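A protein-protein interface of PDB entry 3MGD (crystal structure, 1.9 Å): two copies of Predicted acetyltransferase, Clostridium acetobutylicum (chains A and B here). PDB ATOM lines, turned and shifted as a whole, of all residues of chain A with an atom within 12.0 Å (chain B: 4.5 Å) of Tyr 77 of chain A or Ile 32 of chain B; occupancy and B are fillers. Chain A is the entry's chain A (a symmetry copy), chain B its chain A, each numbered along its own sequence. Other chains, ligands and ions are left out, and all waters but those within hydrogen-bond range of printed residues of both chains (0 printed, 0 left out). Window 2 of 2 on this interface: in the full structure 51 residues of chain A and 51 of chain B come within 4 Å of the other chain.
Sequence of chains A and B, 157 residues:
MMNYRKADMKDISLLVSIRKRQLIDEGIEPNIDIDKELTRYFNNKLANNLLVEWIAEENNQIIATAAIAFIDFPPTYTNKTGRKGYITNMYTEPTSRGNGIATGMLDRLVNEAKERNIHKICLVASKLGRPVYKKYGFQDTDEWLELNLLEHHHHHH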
ATOM      1  N   PHE A  73      -6.692 -27.047  -6.215  1.00  0.00           N
ATOM      2  CA  PHE A  73      -6.503 -28.087  -7.212  1.00  0.00           C
ATOM      3  C   PHE A  73      -6.595 -27.415  -8.586  1.00  0.00           C
ATOM      4  O   PHE A  73      -7.031 -26.272  -8.684  1.00  0.00           O
ATOM      5  CB  PHE A  73      -7.588 -29.162  -7.071  1.00  0.00           C
ATOM      6  CG  PHE A  73      -7.568 -29.886  -5.747  1.00  0.00           C
ATOM      7  CD1 PHE A  73      -6.765 -31.006  -5.560  1.00  0.00           C
ATOM      8  CD2 PHE A  73      -8.355 -29.450  -4.690  1.00  0.00           C
ATOM      9  CE1 PHE A  73      -6.745 -31.683  -4.342  1.00  0.00           C
ATOM     10  CE2 PHE A  73      -8.334 -30.113  -3.469  1.00  0.00           C
ATOM     11  CZ  PHE A  73      -7.532 -31.233  -3.298  1.00  0.00           C
ATOM     12  N   PRO A  74      -6.198 -28.117  -9.656  1.00  0.00           N
ATOM     13  CA  PRO A  74      -6.326 -27.462 -10.962  1.00  0.00           C
ATOM     14  C   PRO A  74      -7.784 -27.172 -11.340  1.00  0.00           C
ATOM     15  O   PRO A  74      -8.654 -28.026 -11.147  1.00  0.00           O
ATOM     16  CB  PRO A  74      -5.741 -28.500 -11.937  1.00  0.00           C
ATOM     17  CG  PRO A  74      -4.886 -29.370 -11.111  1.00  0.00           C
ATOM     18  CD  PRO A  74      -5.542 -29.430  -9.753  1.00  0.00           C
ATOM     19  N   PRO A  75      -8.051 -25.985 -11.910  1.00  0.00           N
ATOM     20  CA  PRO A  75      -9.412 -25.683 -12.363  1.00  0.00           C
ATOM     21  C   PRO A  75      -9.976 -26.740 -13.304  1.00  0.00           C
ATOM     22  O   PRO A  75      -9.246 -27.367 -14.056  1.00  0.00           O
ATOM     23  CB  PRO A  75      -9.241 -24.357 -13.118  1.00  0.00           C
ATOM     24  CG  PRO A  75      -8.107 -23.691 -12.394  1.00  0.00           C
ATOM     25  CD  PRO A  75      -7.155 -24.824 -12.060  1.00  0.00           C
ATOM     26  N   THR A  76     -11.287 -26.942 -13.230  1.00  0.00           N
ATOM     27  CA  THR A  76     -11.980 -27.769 -14.203  1.00  0.00           C
ATOM     28  C   THR A  76     -13.326 -27.125 -14.529  1.00  0.00           C
ATOM     29  O   THR A  76     -13.736 -26.145 -13.887  1.00  0.00           O
ATOM     30  CB  THR A  76     -12.147 -29.212 -13.676  1.00  0.00           C
ATOM     31  OG1 THR A  76     -12.885 -29.987 -14.627  1.00  0.00           O
ATOM     32  CG2 THR A  76     -12.860 -29.201 -12.336  1.00  0.00           C
ATOM     33  N   TYR A  77     -14.018 -27.651 -15.529  1.00  0.00           N
ATOM     34  CA  TYR A  77     -15.261 -27.011 -15.957  1.00  0.00           C
ATOM     35  C   TYR A  77     -16.343 -27.009 -14.883  1.00  0.00           C
ATOM     36  O   TYR A  77     -17.217 -26.149 -14.884  1.00  0.00           O
ATOM     37  CB  TYR A  77     -15.752 -27.638 -17.263  1.00  0.00           C
ATOM     38  CG  TYR A  77     -14.781 -27.355 -18.378  1.00  0.00           C
ATOM     39  CD1 TYR A  77     -14.728 -26.099 -18.980  1.00  0.00           C
ATOM     40  CD2 TYR A  77     -13.875 -28.323 -18.791  1.00  0.00           C
ATOM     41  CE1 TYR A  77     -13.819 -25.833 -19.984  1.00  0.00           C
ATOM     42  CE2 TYR A  77     -12.974 -28.065 -19.790  1.00  0.00           C
ATOM     43  CZ  TYR A  77     -12.955 -26.824 -20.387  1.00  0.00           C
ATOM     44  OH  TYR A  77     -12.048 -26.586 -21.388  1.00  0.00           O
ATOM     45  N   THR A  78     -16.257 -27.953 -13.947  1.00  0.00           N
ATOM     46  CA  THR A  78     -17.250 -28.060 -12.880  1.00  0.00           C
ATOM     47  C   THR A  78     -16.804 -27.406 -11.568  1.00  0.00           C
ATOM     48  O   THR A  78     -17.503 -27.472 -10.562  1.00  0.00           O
ATOM     49  CB  THR A  78     -17.592 -29.527 -12.601  1.00  0.00           C
ATOM     50  OG1 THR A  78     -16.390 -30.245 -12.307  1.00  0.00           O
ATOM     51  CG2 THR A  78     -18.261 -30.149 -13.814  1.00  0.00           C
ATOM     52  N   ASN A  79     -15.636 -26.781 -11.593  1.00  0.00           N
ATOM     53  CA  ASN A  79     -15.096 -26.077 -10.446  1.00  0.00           C
ATOM     54  C   ASN A  79     -14.060 -25.107 -10.983  1.00  0.00           C
ATOM     55  O   ASN A  79     -12.869 -25.391 -10.927  1.00  0.00           O
ATOM     56  CB  ASN A  79     -14.429 -27.090  -9.515  1.00  0.00           C
ATOM     57  CG  ASN A  79     -14.065 -26.505  -8.178  1.00  0.00           C
ATOM     58  OD1 ASN A  79     -13.246 -27.071  -7.430  1.00  0.00           O
ATOM     59  ND2 ASN A  79     -14.667 -25.374  -7.855  1.00  0.00           N
ATOM     60  N   LYS A  80     -14.498 -23.968 -11.524  1.00  0.00           N
ATOM     61  CA  LYS A  80     -13.592 -23.146 -12.334  1.00  0.00           C
ATOM     62  C   LYS A  80     -12.360 -22.590 -11.603  1.00  0.00           C
ATOM     63  O   LYS A  80     -11.345 -22.306 -12.234  1.00  0.00           O
ATOM     64  CB  LYS A  80     -14.354 -22.001 -13.021  1.00  0.00           C
ATOM     65  CG  LYS A  80     -14.932 -20.976 -12.066  1.00  0.00           C
ATOM     66  CD  LYS A  80     -15.585 -19.823 -12.846  1.00  0.00           C
ATOM     67  CE  LYS A  80     -16.127 -18.756 -11.893  1.00  0.00           C
ATOM     68  NZ  LYS A  80     -16.432 -17.462 -12.587  1.00  0.00           N
ATOM     69  N   THR A  81     -12.458 -22.401 -10.292  1.00  0.00           N
ATOM     70  CA  THR A  81     -11.319 -21.890  -9.524  1.00  0.00           C
ATOM     71  C   THR A  81     -10.372 -23.018  -9.087  1.00  0.00           C
ATOM     72  O   THR A  81      -9.210 -22.774  -8.717  1.00  0.00           O
ATOM     73  CB  THR A  81     -11.778 -21.150  -8.238  1.00  0.00           C
ATOM     74  OG1 THR A  81     -12.351 -22.099  -7.337  1.00  0.00           O
ATOM     75  CG2 THR A  81     -12.815 -20.089  -8.552  1.00  0.00           C
ATOM     76  N   GLY A  82     -10.884 -24.240  -9.103  1.00  0.00           N
ATOM     77  CA  GLY A  82     -10.128 -25.391  -8.629  1.00  0.00           C
ATOM     78  C   GLY A  82     -10.043 -25.546  -7.108  1.00  0.00           C
ATOM     79  O   GLY A  82      -9.541 -26.558  -6.602  1.00  0.00           O
ATOM     80  N   ARG A  83     -10.532 -24.550  -6.380  1.00  0.00           N
ATOM     81  CA  ARG A  83     -10.430 -24.568  -4.926  1.00  0.00           C
ATOM     82  C   ARG A  83     -11.459 -25.508  -4.318  1.00  0.00           C
ATOM     83  O   ARG A  83     -12.552 -25.689  -4.857  1.00  0.00           O
ATOM     84  CB  ARG A  83     -10.626 -23.169  -4.340  1.00  0.00           C
ATOM     85  CG  ARG A  83      -9.810 -22.078  -4.997  1.00  0.00           C
ATOM     86  CD  ARG A  83      -9.842 -20.826  -4.141  1.00  0.00           C
ATOM     87  NE  ARG A  83      -9.907 -19.611  -4.947  1.00  0.00           N
ATOM     88  CZ  ARG A  83     -11.038 -19.016  -5.309  1.00  0.00           C
ATOM     89  NH1 ARG A  83     -12.210 -19.527  -4.944  1.00  0.00           N
ATOM     90  NH2 ARG A  83     -10.996 -17.914  -6.046  1.00  0.00           N
ATOM     91  N   LYS A  84     -11.095 -26.097  -3.180  1.00  0.00           N
ATOM     92  CA  LYS A  84     -12.010 -26.926  -2.416  1.00  0.00           C
ATOM     93  C   LYS A  84     -11.827 -26.647  -0.940  1.00  0.00           C
ATOM     94  O   LYS A  84     -10.754 -26.228  -0.511  1.00  0.00           O
ATOM     95  CB  LYS A  84     -11.747 -28.417  -2.677  1.00  0.00           C
ATOM     96  CG  LYS A  84     -12.248 -28.914  -4.054  1.00  0.00           C
ATOM     97  CD  LYS A  84     -12.065 -30.426  -4.195  1.00  0.00           C
ATOM     98  CE  LYS A  84     -12.736 -30.970  -5.452  1.00  0.00           C
ATOM     99  NZ  LYS A  84     -12.519 -32.438  -5.579  1.00  0.00           N
ATOM    100  N   ASN A 117     -16.249 -18.121  -1.796  1.00  0.00           N
ATOM    101  CA  ASN A 117     -16.602 -18.556  -3.144  1.00  0.00           C
ATOM    102  C   ASN A 117     -16.154 -19.979  -3.472  1.00  0.00           C
ATOM    103  O   ASN A 117     -15.668 -20.267  -4.575  1.00  0.00           O
ATOM    104  CB  ASN A 117     -16.073 -17.564  -4.190  1.00  0.00           C
ATOM    105  CG  ASN A 117     -16.767 -16.214  -4.105  1.00  0.00           C
ATOM    106  OD1 ASN A 117     -17.911 -16.125  -3.659  1.00  0.00           O
ATOM    107  ND2 ASN A 117     -16.082 -15.156  -4.539  1.00  0.00           N
ATOM    108  N   HIS A 119     -17.483 -24.008  -3.533  1.00  0.00           N
ATOM    109  CA  HIS A 119     -18.727 -24.771  -3.572  1.00  0.00           C
ATOM    110  C   HIS A 119     -18.511 -26.277  -3.622  1.00  0.00           C
ATOM    111  O   HIS A 119     -19.464 -27.042  -3.741  1.00  0.00           O
ATOM    112  CB  HIS A 119     -19.610 -24.313  -4.738  1.00  0.00           C
ATOM    113  CG  HIS A 119     -18.968 -24.465  -6.084  1.00  0.00           C
ATOM    114  ND1 HIS A 119     -19.090 -25.611  -6.838  1.00  0.00           N
ATOM    115  CD2 HIS A 119     -18.200 -23.618  -6.808  1.00  0.00           C
ATOM    116  CE1 HIS A 119     -18.423 -25.465  -7.970  1.00  0.00           C
ATOM    117  NE2 HIS A 119     -17.873 -24.264  -7.976  1.00  0.00           N
ATOM    118  N   LYS A 120     -17.262 -26.702  -3.523  1.00  0.00           N
ATOM    119  CA  LYS A 120     -16.955 -28.126  -3.447  1.00  0.00           C
ATOM    120  C   LYS A 120     -16.205 -28.400  -2.148  1.00  0.00           C
ATOM    121  O   LYS A 120     -15.179 -27.775  -1.885  1.00  0.00           O
ATOM    122  CB  LYS A 120     -16.092 -28.561  -4.636  1.00  0.00           C
ATOM    123  CG  LYS A 120     -16.763 -28.434  -6.009  1.00  0.00           C
ATOM    124  CD  LYS A 120     -17.651 -29.630  -6.309  1.00  0.00           C
ATOM    125  CE  LYS A 120     -18.352 -29.485  -7.672  1.00  0.00           C
ATOM    126  NZ  LYS A 120     -19.352 -28.371  -7.663  1.00  0.00           N
ATOM    127  N   LYS B  20      -7.107 -28.699 -21.151  1.00  0.00           N
ATOM    128  CA  LYS B  20      -8.458 -28.705 -21.716  1.00  0.00           C
ATOM    129  C   LYS B  20      -8.683 -29.927 -22.607  1.00  0.00           C
ATOM    130  O   LYS B  20      -9.731 -30.579 -22.545  1.00  0.00           O
ATOM    131  CB  LYS B  20      -8.738 -27.416 -22.502  1.00  0.00           C
ATOM    132  CG  LYS B  20      -8.805 -26.152 -21.653  1.00  0.00           C
ATOM    133  CD  LYS B  20      -9.288 -24.932 -22.446  1.00  0.00           C
ATOM    134  CE  LYS B  20      -8.306 -24.521 -23.507  1.00  0.00           C
ATOM    135  NZ  LYS B  20      -8.657 -23.191 -24.138  1.00  0.00           N
ATOM    136  N   LEU B  23      -9.231 -33.018 -20.441  1.00  0.00           N
ATOM    137  CA  LEU B  23     -10.524 -33.073 -19.780  1.00  0.00           C
ATOM    138  C   LEU B  23     -11.616 -33.420 -20.779  1.00  0.00           C
ATOM    139  O   LEU B  23     -12.540 -34.166 -20.479  1.00  0.00           O
ATOM    140  CB  LEU B  23     -10.832 -31.730 -19.127  1.00  0.00           C
ATOM    141  CG  LEU B  23      -9.912 -31.301 -17.980  1.00  0.00           C
ATOM    142  CD1 LEU B  23     -10.241 -29.884 -17.572  1.00  0.00           C
ATOM    143  CD2 LEU B  23     -10.022 -32.260 -16.767  1.00  0.00           C
ATOM    144  N   ILE B  28     -15.683 -34.641 -20.199  1.00  0.00           N
ATOM    145  CA  ILE B  28     -16.266 -33.496 -19.508  1.00  0.00           C
ATOM    146  C   ILE B  28     -16.842 -32.496 -20.516  1.00  0.00           C
ATOM    147  O   ILE B  28     -16.343 -32.368 -21.642  1.00  0.00           O
ATOM    148  CB  ILE B  28     -15.259 -32.860 -18.517  1.00  0.00           C
ATOM    149  CG1 ILE B  28     -14.896 -33.899 -17.446  1.00  0.00           C
ATOM    150  CG2 ILE B  28     -15.847 -31.627 -17.850  1.00  0.00           C
ATOM    151  CD1 ILE B  28     -13.583 -33.654 -16.738  1.00  0.00           C
ATOM    152  N   GLU B  29     -17.925 -31.827 -20.126  1.00  0.00           N
ATOM    153  CA  GLU B  29     -18.570 -30.857 -20.998  1.00  0.00           C
ATOM    154  C   GLU B  29     -17.957 -29.472 -20.819  1.00  0.00           C
ATOM    155  O   GLU B  29     -18.108 -28.842 -19.761  1.00  0.00           O
ATOM    156  CB  GLU B  29     -20.089 -30.851 -20.780  1.00  0.00           C
ATOM    157  CG  GLU B  29     -20.772 -32.100 -21.338  1.00  0.00           C
ATOM    158  CD  GLU B  29     -22.236 -32.216 -20.937  1.00  0.00           C
ATOM    159  OE1 GLU B  29     -22.846 -31.188 -20.575  1.00  0.00           O
ATOM    160  OE2 GLU B  29     -22.777 -33.341 -20.991  1.00  0.00           O
ATOM    161  N   PRO B  30     -17.245 -28.998 -21.859  1.00  0.00           N
ATOM    162  CA  PRO B  30     -16.508 -27.732 -21.813  1.00  0.00           C
ATOM    163  C   PRO B  30     -17.434 -26.527 -21.994  1.00  0.00           C
ATOM    164  O   PRO B  30     -17.310 -25.780 -22.955  1.00  0.00           O
ATOM    165  CB  PRO B  30     -15.519 -27.872 -22.974  1.00  0.00           C
ATOM    166  CG  PRO B  30     -16.249 -28.707 -23.961  1.00  0.00           C
ATOM    167  CD  PRO B  30     -17.079 -29.683 -23.158  1.00  0.00           C
ATOM    168  N   ASN B  31     -18.291 -26.346 -20.986  1.00  0.00           N
ATOM    169  CA  ASN B  31     -19.470 -25.487 -20.932  1.00  0.00           C
ATOM    170  C   ASN B  31     -19.182 -24.022 -20.710  1.00  0.00           C
ATOM    171  O   ASN B  31     -20.020 -23.168 -20.965  1.00  0.00           O
ATOM    172  CB  ASN B  31     -20.262 -25.907 -19.689  1.00  0.00           C
ATOM    173  CG  ASN B  31     -21.509 -26.639 -20.018  1.00  0.00           C
ATOM    174  OD1 ASN B  31     -22.056 -26.492 -21.110  1.00  0.00           O
ATOM    175  ND2 ASN B  31     -21.993 -27.427 -19.070  1.00  0.00           N
ATOM    176  N   ILE B  32     -18.025 -23.745 -20.132  1.00  0.00           N
ATOM    177  CA  ILE B  32     -17.683 -22.389 -19.742  1.00  0.00           C
ATOM    178  C   ILE B  32     -16.221 -22.200 -20.095  1.00  0.00           C
ATOM    179  O   ILE B  32     -15.518 -23.168 -20.349  1.00  0.00           O
ATOM    180  CB  ILE B  32     -17.906 -22.152 -18.224  1.00  0.00           C
ATOM    181  CG1 ILE B  32     -17.055 -23.114 -17.401  1.00  0.00           C
ATOM    182  CG2 ILE B  32     -19.375 -22.327 -17.859  1.00  0.00           C
ATOM    183  CD1 ILE B  32     -17.124 -22.871 -15.893  1.00  0.00           C
ATOM    184  N   ASP B  33     -15.783 -20.951 -20.138  1.00  0.00           N
ATOM    185  CA  ASP B  33     -14.414 -20.625 -20.503  1.00  0.00           C
ATOM    186  C   ASP B  33     -13.593 -20.583 -19.221  1.00  0.00           C
ATOM    187  O   ASP B  33     -13.843 -19.733 -18.372  1.00  0.00           O
ATOM    188  CB  ASP B  33     -14.400 -19.246 -21.132  1.00  0.00           C
ATOM    189  CG  ASP B  33     -13.037 -18.855 -21.662  1.00  0.00           C
ATOM    190  OD1 ASP B  33     -12.033 -19.403 -21.180  1.00  0.00           O
ATOM    191  OD2 ASP B  33     -12.967 -17.991 -22.565  1.00  0.00           O
ATOM    192  N   ILE B  34     -12.621 -21.475 -19.069  1.00  0.00           N
ATOM    193  CA  ILE B  34     -11.777 -21.429 -17.868  1.00  0.00           C
ATOM    194  C   ILE B  34     -10.322 -21.067 -18.180  1.00  0.00           C
ATOM    195  O   ILE B  34      -9.421 -21.340 -17.394  1.00  0.00           O
ATOM    196  CB  ILE B  34     -11.833 -22.736 -17.058  1.00  0.00           C
ATOM    197  CG1 ILE B  34     -11.336 -23.915 -17.898  1.00  0.00           C
ATOM    198  CG2 ILE B  34     -13.258 -22.974 -16.515  1.00  0.00           C
ATOM    199  CD1 ILE B  34     -11.246 -25.202 -17.113  1.00  0.00           C
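Ile 32 of chain B touches just one residue of chain A: Tyr 77. Lys 20 of chain B touches just one residue of chain A: Tyr 77 (3.3 Å). Leu 23 of chain B touches just these residues of chain A: Thr 76 (3.96 Å) and Tyr 77 (3.96 Å). Ile 28 of chain B touches just one residue of chain A: Tyr 77 (3.96 Å). Pro 30 of chain B touches one residue of chain A. Of the printed residues of chain B, Lys 80 of chain A touches Ile 34 (3.8 Å). Of the printed residues of chain A, Glu 29 of chain B touches Tyr 77. Of the printed residues of chain B, Thr 76 of chain A touches Leu 23 (3.96 Å) and Ile 34 (3.8 Å). Arg 83 of chain A touches none of the printed residues of chain B. Pro 75 of chain A touches none of the printed residues of chain B. The nearest residue of chain B that does not touch Tyr 77 of chain A is Asn 31 of chain B (4.1 Å).
No position is printed for both chains. Of the 10 pairs that touch across the chains among the printed residues, none has its exchanged pair printed and touching as well.
Of the 9 printed residues of chain B, 7 touch a printed residue of chain A. Printed residues of chain B that touch a printed residue of chain A: Lys 20, Leu 23, Ile 28, Glu 29, Pro 30, Ile 32 and Ile 34. Hydrophobic or aromatic side chains of chain A that line the printed part of chain B: Tyr 77. Among the printed residues, no Asp or Glu carboxylate lies within 4 Å of a Lys or Arg side-chain nitrogen of the other chain.
Leu 23 of chain B touches Thr 76 of chain A (CD1 to OG1, 3.96 Å). Thr 76 of chain A touches Ile 34 of chain B (C to CD1, 3.8 Å). OH of Tyr 77 of chain A touches CG of Lys 20 of chain B (3.3 Å). CE2 of Tyr 77 of chain A touches CD1 of Leu 23 of chain B, 3.96 Å away. Ile 28 of chain B touches Tyr 77 of chain A. Tyr 77 of chain A touches Glu 29 of chain B (CB to O, 3.6 Å). Pro 30 of chain B touches Tyr 77 of chain A. CE1 of Tyr 77 of chain A touches O of Ile 32 of chain B (3.2 Å). Tyr 77 of chain A touches Ile 34 of chain B. Lys 80 of chain A touches Ile 34 of chain B.
The backbone NH of Ile 28 of chain B sits at hydrogen-bond distance from the backbone carbonyl oxygen of Leu 23 of chain B.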
